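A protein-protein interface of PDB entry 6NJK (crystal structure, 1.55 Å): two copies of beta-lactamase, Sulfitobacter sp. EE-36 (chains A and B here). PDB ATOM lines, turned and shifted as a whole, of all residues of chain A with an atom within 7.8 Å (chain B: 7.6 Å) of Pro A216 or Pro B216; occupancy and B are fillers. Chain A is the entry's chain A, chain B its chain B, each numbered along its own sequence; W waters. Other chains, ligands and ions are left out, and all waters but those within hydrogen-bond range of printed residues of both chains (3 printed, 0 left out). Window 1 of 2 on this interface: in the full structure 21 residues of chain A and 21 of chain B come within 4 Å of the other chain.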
ATOM      1  N   VAL A 128      -5.934  32.010 -11.386  1.00  0.00           N
ATOM      2  CA  VAL A 128      -7.310  32.145 -11.849  1.00  0.00           C
ATOM      3  C   VAL A 128      -8.226  31.417 -10.873  1.00  0.00           C
ATOM      4  O   VAL A 128      -8.022  30.232 -10.581  1.00  0.00           O
ATOM      5  CB  VAL A 128      -7.476  31.594 -13.277  1.00  0.00           C
ATOM      6  CG1 VAL A 128      -8.943  31.492 -13.623  1.00  0.00           C
ATOM      7  CG2 VAL A 128      -6.736  32.482 -14.265  1.00  0.00           C
ATOM      8  N   GLY A 129      -9.246  32.119 -10.385  1.00  0.00           N
ATOM      9  CA  GLY A 129     -10.071  31.588  -9.317  1.00  0.00           C
ATOM     10  C   GLY A 129     -11.513  31.307  -9.686  1.00  0.00           C
ATOM     11  O   GLY A 129     -12.250  30.713  -8.892  1.00  0.00           O
ATOM     12  N   ASN A 130     -11.935  31.746 -10.869  1.00  0.00           N
ATOM     13  CA  ASN A 130     -13.275  31.469 -11.374  1.00  0.00           C
ATOM     14  C   ASN A 130     -13.285  31.773 -12.868  1.00  0.00           C
ATOM     15  O   ASN A 130     -12.294  32.241 -13.434  1.00  0.00           O
ATOM     16  CB  ASN A 130     -14.362  32.259 -10.607  1.00  0.00           C
ATOM     17  CG  ASN A 130     -14.224  33.782 -10.719  1.00  0.00           C
ATOM     18  OD1 ASN A 130     -13.373  34.304 -11.439  1.00  0.00           O
ATOM     19  ND2 ASN A 130     -15.087  34.500  -9.998  1.00  0.00           N
ATOM     20  N   VAL A 131     -14.413  31.470 -13.513  1.00  0.00           N
ATOM     21  CA  VAL A 131     -14.460  31.642 -14.962  1.00  0.00           C
ATOM     22  C   VAL A 131     -14.338  33.116 -15.348  1.00  0.00           C
ATOM     23  O   VAL A 131     -13.744  33.447 -16.381  1.00  0.00           O
ATOM     24  CB  VAL A 131     -15.737  31.014 -15.543  1.00  0.00           C
ATOM     25  CG1 VAL A 131     -15.859  31.352 -17.014  1.00  0.00           C
ATOM     26  CG2 VAL A 131     -15.711  29.508 -15.368  1.00  0.00           C
ATOM     27  N   ARG A 213     -10.310  10.947  -4.304  1.00  0.00           N
ATOM     28  CA  ARG A 213     -11.568  11.424  -4.863  1.00  0.00           C
ATOM     29  C   ARG A 213     -11.324  12.722  -5.616  1.00  0.00           C
ATOM     30  O   ARG A 213     -10.659  13.620  -5.092  1.00  0.00           O
ATOM     31  CB  ARG A 213     -12.579  11.634  -3.726  1.00  0.00           C
ATOM     32  CG  ARG A 213     -13.859  12.323  -4.111  1.00  0.00           C
ATOM     33  CD  ARG A 213     -14.656  11.429  -5.023  1.00  0.00           C
ATOM     34  NE  ARG A 213     -15.275  10.319  -4.299  1.00  0.00           N
ATOM     35  CZ  ARG A 213     -15.330   9.062  -4.737  1.00  0.00           C
ATOM     36  NH1 ARG A 213     -14.769   8.718  -5.889  1.00  0.00           N
ATOM     37  NH2 ARG A 213     -15.934   8.133  -4.006  1.00  0.00           N
ATOM     38  N   VAL A 214     -11.881  12.832  -6.828  1.00  0.00           N
ATOM     39  CA  VAL A 214     -11.712  14.051  -7.611  1.00  0.00           C
ATOM     40  C   VAL A 214     -12.330  15.221  -6.856  1.00  0.00           C
ATOM     41  O   VAL A 214     -13.408  15.105  -6.258  1.00  0.00           O
ATOM     42  CB  VAL A 214     -12.313  13.888  -9.019  1.00  0.00           C
ATOM     43  CG1 VAL A 214     -13.831  13.767  -8.986  1.00  0.00           C
ATOM     44  CG2 VAL A 214     -11.888  15.055  -9.903  1.00  0.00           C
ATOM     45  N   ASN A 215     -11.632  16.350  -6.857  1.00  0.00           N
ATOM     46  CA  ASN A 215     -12.030  17.505  -6.068  1.00  0.00           C
ATOM     47  C   ASN A 215     -12.571  18.623  -6.956  1.00  0.00           C
ATOM     48  O   ASN A 215     -12.321  18.651  -8.165  1.00  0.00           O
ATOM     49  CB  ASN A 215     -10.844  18.039  -5.248  1.00  0.00           C
ATOM     50  CG  ASN A 215     -10.231  16.985  -4.321  1.00  0.00           C
ATOM     51  OD1 ASN A 215      -9.005  16.866  -4.233  1.00  0.00           O
ATOM     52  ND2 ASN A 215     -11.079  16.225  -3.626  1.00  0.00           N
ATOM     53  N   PRO A 216     -13.336  19.555  -6.379  1.00  0.00           N
ATOM     54  CA  PRO A 216     -13.816  20.717  -7.139  1.00  0.00           C
ATOM     55  C   PRO A 216     -12.660  21.527  -7.704  1.00  0.00           C
ATOM     56  O   PRO A 216     -11.540  21.495  -7.195  1.00  0.00           O
ATOM     57  CB  PRO A 216     -14.601  21.528  -6.095  1.00  0.00           C
ATOM     58  CG  PRO A 216     -15.004  20.529  -5.061  1.00  0.00           C
ATOM     59  CD  PRO A 216     -13.917  19.489  -5.026  1.00  0.00           C
ATOM     60  N   GLY A 217     -12.947  22.267  -8.769  1.00  0.00           N
ATOM     61  CA  GLY A 217     -11.954  23.137  -9.376  1.00  0.00           C
ATOM     62  C   GLY A 217     -12.632  24.023 -10.392  1.00  0.00           C
ATOM     63  O   GLY A 217     -13.788  23.801 -10.763  1.00  0.00           O
ATOM     64  N   VAL A 218     -11.903  25.045 -10.842  1.00  0.00           N
ATOM     65  CA  VAL A 218     -12.443  25.910 -11.881  1.00  0.00           C
ATOM     66  C   VAL A 218     -12.663  25.078 -13.138  1.00  0.00           C
ATOM     67  O   VAL A 218     -11.749  24.399 -13.621  1.00  0.00           O
ATOM     68  CB  VAL A 218     -11.507  27.097 -12.144  1.00  0.00           C
ATOM     69  CG1 VAL A 218     -12.040  27.953 -13.301  1.00  0.00           C
ATOM     70  CG2 VAL A 218     -11.347  27.940 -10.891  1.00  0.00           C
ATOM     71  N   LEU A 219     -13.881  25.125 -13.669  1.00  0.00           N
ATOM     72  CA  LEU A 219     -14.276  24.400 -14.877  1.00  0.00           C
ATOM     73  C   LEU A 219     -14.202  22.887 -14.698  1.00  0.00           C
ATOM     74  O   LEU A 219     -14.224  22.144 -15.685  1.00  0.00           O
ATOM     75  CB  LEU A 219     -13.437  24.804 -16.099  1.00  0.00           C
ATOM     76  CG  LEU A 219     -13.603  26.233 -16.616  1.00  0.00           C
ATOM     77  CD1 LEU A 219     -12.698  26.473 -17.827  1.00  0.00           C
ATOM     78  CD2 LEU A 219     -15.054  26.532 -16.968  1.00  0.00           C
ATOM     79  N   ALA A 220     -14.134  22.404 -13.454  1.00  0.00           N
ATOM     80  CA  ALA A 220     -14.087  20.962 -13.243  1.00  0.00           C
ATOM     81  C   ALA A 220     -15.368  20.295 -13.727  1.00  0.00           C
ATOM     82  O   ALA A 220     -15.318  19.250 -14.384  1.00  0.00           O
ATOM     83  CB  ALA A 220     -13.849  20.652 -11.765  1.00  0.00           C
ATOM     84  N   ASP A 221     -16.528  20.882 -13.426  1.00  0.00           N
ATOM     85  CA  ASP A 221     -17.775  20.271 -13.876  1.00  0.00           C
ATOM     86  C   ASP A 221     -17.776  20.097 -15.389  1.00  0.00           C
ATOM     87  O   ASP A 221     -18.209  19.060 -15.909  1.00  0.00           O
ATOM     88  CB  ASP A 221     -18.971  21.121 -13.460  1.00  0.00           C
ATOM     89  CG  ASP A 221     -19.319  20.973 -11.997  1.00  0.00           C
ATOM     90  OD1 ASP A 221     -18.669  20.168 -11.290  1.00  0.00           O
ATOM     91  OD2 ASP A 221     -20.254  21.678 -11.557  1.00  0.00           O
ATOM     92  N   TYR A 224     -14.118  17.691 -16.489  1.00  0.00           N
ATOM     93  CA  TYR A 224     -13.882  16.346 -15.969  1.00  0.00           C
ATOM     94  C   TYR A 224     -14.884  16.018 -14.866  1.00  0.00           C
ATOM     95  O   TYR A 224     -14.565  15.314 -13.903  1.00  0.00           O
ATOM     96  CB  TYR A 224     -12.438  16.172 -15.474  1.00  0.00           C
ATOM     97  CG  TYR A 224     -11.888  17.257 -14.562  1.00  0.00           C
ATOM     98  CD1 TYR A 224     -11.977  17.144 -13.179  1.00  0.00           C
ATOM     99  CD2 TYR A 224     -11.250  18.375 -15.086  1.00  0.00           C
ATOM    100  CE1 TYR A 224     -11.472  18.130 -12.346  1.00  0.00           C
ATOM    101  CE2 TYR A 224     -10.739  19.361 -14.262  1.00  0.00           C
ATOM    102  CZ  TYR A 224     -10.849  19.232 -12.896  1.00  0.00           C
ATOM    103  OH  TYR A 224     -10.331  20.214 -12.086  1.00  0.00           O
ATOM    104  N   LYS A 227     -19.570  11.394 -13.655  1.00  0.00           N
ATOM    105  CA  LYS A 227     -19.399  10.088 -13.033  1.00  0.00           C
ATOM    106  C   LYS A 227     -20.512   9.194 -13.562  1.00  0.00           C
ATOM    107  O   LYS A 227     -21.659   9.634 -13.661  1.00  0.00           O
ATOM    108  CB  LYS A 227     -19.454  10.198 -11.500  1.00  0.00           C
ATOM    109  CG  LYS A 227     -18.394  11.134 -10.924  1.00  0.00           C
ATOM    110  CD  LYS A 227     -18.908  12.551 -10.776  1.00  0.00           C
ATOM    111  CE  LYS A 227     -17.800  13.499 -10.316  1.00  0.00           C
ATOM    112  NZ  LYS A 227     -18.269  14.909 -10.183  1.00  0.00           N
ATOM    113  N   VAL B 128     -13.304  12.848   0.323  1.00  0.00           N
ATOM    114  CA  VAL B 128     -14.653  13.395   0.247  1.00  0.00           C
ATOM    115  C   VAL B 128     -14.694  14.391  -0.900  1.00  0.00           C
ATOM    116  O   VAL B 128     -13.850  15.293  -0.974  1.00  0.00           O
ATOM    117  CB  VAL B 128     -15.055  14.060   1.575  1.00  0.00           C
ATOM    118  CG1 VAL B 128     -16.244  14.988   1.385  1.00  0.00           C
ATOM    119  CG2 VAL B 128     -15.340  12.996   2.617  1.00  0.00           C
ATOM    120  N   GLY B 129     -15.685  14.251  -1.774  1.00  0.00           N
ATOM    121  CA  GLY B 129     -15.699  15.034  -2.990  1.00  0.00           C
ATOM    122  C   GLY B 129     -16.820  16.043  -3.103  1.00  0.00           C
ATOM    123  O   GLY B 129     -16.819  16.860  -4.030  1.00  0.00           O
ATOM    124  N   ASN B 130     -17.789  15.980  -2.192  1.00  0.00           N
ATOM    125  CA  ASN B 130     -18.885  16.942  -2.141  1.00  0.00           C
ATOM    126  C   ASN B 130     -19.552  16.827  -0.773  1.00  0.00           C
ATOM    127  O   ASN B 130     -19.160  16.013   0.069  1.00  0.00           O
ATOM    128  CB  ASN B 130     -19.883  16.755  -3.299  1.00  0.00           C
ATOM    129  CG  ASN B 130     -20.576  15.400  -3.308  1.00  0.00           C
ATOM    130  OD1 ASN B 130     -20.379  14.571  -2.423  1.00  0.00           O
ATOM    131  ND2 ASN B 130     -21.427  15.188  -4.314  1.00  0.00           N
ATOM    132  N   ARG B 213      -4.351  32.301  -6.231  1.00  0.00           N
ATOM    133  CA  ARG B 213      -5.760  32.622  -6.051  1.00  0.00           C
ATOM    134  C   ARG B 213      -6.420  31.469  -5.315  1.00  0.00           C
ATOM    135  O   ARG B 213      -6.141  30.305  -5.612  1.00  0.00           O
ATOM    136  CB  ARG B 213      -6.410  32.864  -7.426  1.00  0.00           C
ATOM    137  CG  ARG B 213      -7.882  33.173  -7.436  1.00  0.00           C
ATOM    138  CD  ARG B 213      -8.158  34.488  -6.752  1.00  0.00           C
ATOM    139  NE  ARG B 213      -7.801  35.644  -7.571  1.00  0.00           N
ATOM    140  CZ  ARG B 213      -7.331  36.791  -7.084  1.00  0.00           C
ATOM    141  NH1 ARG B 213      -7.127  36.936  -5.778  1.00  0.00           N
ATOM    142  NH2 ARG B 213      -7.055  37.789  -7.911  1.00  0.00           N
ATOM    143  N   VAL B 214      -7.280  31.792  -4.343  1.00  0.00           N
ATOM    144  CA  VAL B 214      -8.016  30.751  -3.638  1.00  0.00           C
ATOM    145  C   VAL B 214      -8.885  30.016  -4.648  1.00  0.00           C
ATOM    146  O   VAL B 214      -9.525  30.630  -5.514  1.00  0.00           O
ATOM    147  CB  VAL B 214      -8.855  31.343  -2.492  1.00  0.00           C
ATOM    148  CG1 VAL B 214      -9.964  32.237  -3.025  1.00  0.00           C
ATOM    149  CG2 VAL B 214      -9.444  30.237  -1.623  1.00  0.00           C
ATOM    150  N   ASN B 215      -8.890  28.691  -4.561  1.00  0.00           N
ATOM    151  CA  ASN B 215      -9.587  27.876  -5.543  1.00  0.00           C
ATOM    152  C   ASN B 215     -10.814  27.195  -4.949  1.00  0.00           C
ATOM    153  O   ASN B 215     -10.978  27.118  -3.726  1.00  0.00           O
ATOM    154  CB  ASN B 215      -8.650  26.813  -6.145  1.00  0.00           C
ATOM    155  CG  ASN B 215      -7.728  26.176  -5.113  1.00  0.00           C
ATOM    156  OD1 ASN B 215      -7.082  26.871  -4.326  1.00  0.00           O
ATOM    157  ND2 ASN B 215      -7.659  24.847  -5.121  1.00  0.00           N
ATOM    158  N   PRO B 216     -11.721  26.722  -5.805  1.00  0.00           N
ATOM    159  CA  PRO B 216     -12.899  25.995  -5.322  1.00  0.00           C
ATOM    160  C   PRO B 216     -12.523  24.771  -4.503  1.00  0.00           C
ATOM    161  O   PRO B 216     -11.453  24.180  -4.655  1.00  0.00           O
ATOM    162  CB  PRO B 216     -13.621  25.586  -6.617  1.00  0.00           C
ATOM    163  CG  PRO B 216     -13.166  26.579  -7.633  1.00  0.00           C
ATOM    164  CD  PRO B 216     -11.753  26.931  -7.265  1.00  0.00           C
ATOM    165  N   GLY B 217     -13.448  24.369  -3.644  1.00  0.00           N
ATOM    166  CA  GLY B 217     -13.235  23.210  -2.798  1.00  0.00           C
ATOM    167  C   GLY B 217     -14.524  22.885  -2.088  1.00  0.00           C
ATOM    168  O   GLY B 217     -15.478  23.668  -2.104  1.00  0.00           O
ATOM    169  N   VAL B 218     -14.558  21.707  -1.469  1.00  0.00           N
ATOM    170  CA  VAL B 218     -15.756  21.325  -0.742  1.00  0.00           C
ATOM    171  C   VAL B 218     -15.941  22.293   0.416  1.00  0.00           C
ATOM    172  O   VAL B 218     -15.027  22.499   1.226  1.00  0.00           O
ATOM    173  CB  VAL B 218     -15.683  19.873  -0.239  1.00  0.00           C
ATOM    174  CG1 VAL B 218     -16.938  19.556   0.587  1.00  0.00           C
ATOM    175  CG2 VAL B 218     -15.531  18.920  -1.409  1.00  0.00           C
ATOM    176  N   LEU B 219     -17.114  22.915   0.482  1.00  0.00           N
ATOM    177  CA  LEU B 219     -17.459  23.874   1.526  1.00  0.00           C
ATOM    178  C   LEU B 219     -16.602  25.136   1.484  1.00  0.00           C
ATOM    179  O   LEU B 219     -16.566  25.901   2.458  1.00  0.00           O
ATOM    180  CB  LEU B 219     -17.375  23.232   2.918  1.00  0.00           C
ATOM    181  CG  LEU B 219     -18.470  22.206   3.227  1.00  0.00           C
ATOM    182  CD1 LEU B 219     -18.267  21.632   4.606  1.00  0.00           C
ATOM    183  CD2 LEU B 219     -19.847  22.842   3.109  1.00  0.00           C
ATOM    184  N   ALA B 220     -15.945  25.410   0.356  1.00  0.00           N
ATOM    185  CA  ALA B 220     -15.104  26.597   0.280  1.00  0.00           C
ATOM    186  C   ALA B 220     -15.920  27.878   0.395  1.00  0.00           C
ATOM    187  O   ALA B 220     -15.508  28.824   1.084  1.00  0.00           O
ATOM    188  CB  ALA B 220     -14.317  26.596  -1.028  1.00  0.00           C
ATOM    189  N   ASP B 221     -17.062  27.947  -0.295  1.00  0.00           N
ATOM    190  CA  ASP B 221     -17.888  29.147  -0.226  1.00  0.00           C
ATOM    191  C   ASP B 221     -18.293  29.435   1.212  1.00  0.00           C
ATOM    192  O   ASP B 221     -18.281  30.589   1.657  1.00  0.00           O
ATOM    193  CB  ASP B 221     -19.141  28.984  -1.091  1.00  0.00           C
ATOM    194  CG  ASP B 221     -18.870  29.129  -2.590  1.00  0.00           C
ATOM    195  OD1 ASP B 221     -17.726  29.435  -2.994  1.00  0.00           O
ATOM    196  OD2 ASP B 221     -19.825  28.938  -3.376  1.00  0.00           O
ATOM    197  N   TYR B 224     -14.568  29.763   3.629  1.00  0.00           N
ATOM    198  CA  TYR B 224     -13.518  30.731   3.330  1.00  0.00           C
ATOM    199  C   TYR B 224     -13.780  31.413   1.994  1.00  0.00           C
ATOM    200  O   TYR B 224     -12.848  31.762   1.262  1.00  0.00           O
ATOM    201  CB  TYR B 224     -12.123  30.082   3.361  1.00  0.00           C
ATOM    202  CG  TYR B 224     -11.956  28.779   2.602  1.00  0.00           C
ATOM    203  CD1 TYR B 224     -11.545  28.773   1.274  1.00  0.00           C
ATOM    204  CD2 TYR B 224     -12.166  27.556   3.224  1.00  0.00           C
ATOM    205  CE1 TYR B 224     -11.379  27.588   0.574  1.00  0.00           C
ATOM    206  CE2 TYR B 224     -12.004  26.361   2.533  1.00  0.00           C
ATOM    207  CZ  TYR B 224     -11.604  26.384   1.207  1.00  0.00           C
ATOM    208  OH  TYR B 224     -11.438  25.203   0.507  1.00  0.00           O
HETATM  209  O   HOH W   1     -11.605  31.694  -6.157  1.00  0.00           O
HETATM  210  O   HOH W   2     -15.900  15.551  -6.428  1.00  0.00           O
HETATM  211  O   HOH W   3      -9.432  23.710  -6.674  1.00  0.00           O
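The backbone carbonyl oxygen (O) of Arg A213 lies within hydrogen-bond range of the side-chain amide nitrogen (ND2) of Asn A215 (3.0 Å).
Among the printed residues, pairs that only touch across the chains: Gly A129 with Arg B213 (3.3 Å), Arg A213 with Gly B129 (3.5 Å), Pro A216 with Pro B216 (3.7 Å), Val A218 with Pro B216 (3.8 Å), Gly A217 with Pro B216 (3.8 Å), Pro A216 with Val B218 (3.8 Å), Pro A216 with Gly B217 (3.8 Å), Val A128 with Arg B213 (3.9 Å), Arg A213 with Val B128 (3.9 Å), Asn A215 with Val B128 (3.9 Å), Gly A129 with Val B214 (3.96 Å) and Val A214 with Gly B129 (3.99 Å).
Of the printed residues of chain B, Val A128 touches Arg B213 (3.9 Å). Printed residues of chain B within 4 Å of Gly A129: Arg B213 and Val B214. Lys A227 touches none of the printed residues of chain B. Of the printed residues of chain A, Val B128 touches Arg A213 and Asn A215. Asn B215 touches none of the printed residues of chain A. Pro B216 touches three residues of chain A. The nearest residue of chain B that does not touch Pro A216 is Gly B129 (4.04 Å). The nearest residue of chain A that does not touch Pro B216 is Gly A129 (4.1 Å).
Of the 15 printed residues of chain A, 8 touch a printed residue of chain B. Hydrophobic or aromatic side chains of chain A within 4 Å of the printed part of chain B: Pro A216 and Val A218. Of the 13 printed residues of chain B, 7 touch a printed residue of chain A. Along chain B the printed residues that touch a printed residue of chain A span positions 128 to 218. Among the printed residues, 12 pairs touch across the chains. Among the printed residues, no Asp or Glu carboxylate lies within 4 Å of a Lys or Arg side-chain nitrogen of the other chain.
Gly A129 touches Val B214, and with the chains exchanged Val A214 touches Gly B129. Asn A215 touches Val B128, but with the chains exchanged Val A128 does not touch Asn B215 (5.6 Å). Pro B216 touches its own counterpart, Pro A216. Pro A216 touches Gly B217, and with the chains exchanged Gly A217 touches Pro B216. Positions printed for both chains: 128, 129, 130, 213, 214, 215, 216, 217, 218, 219, 220, 221 and 224.
Water W1 bridges the backbone carbonyl oxygen (O) of Val B214 and the backbone carbonyl oxygen (O) of Gly A129. Water W2 lies within hydrogen-bond range of O of Val A214 (2.5 Å) and O of Gly B129 (2.9 Å). Water W3 lies within hydrogen-bond range of ND2 of Asn B215 (2.6 Å), O of Pro B216 (2.9 Å) and O of Pro A216 (3.1 Å).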
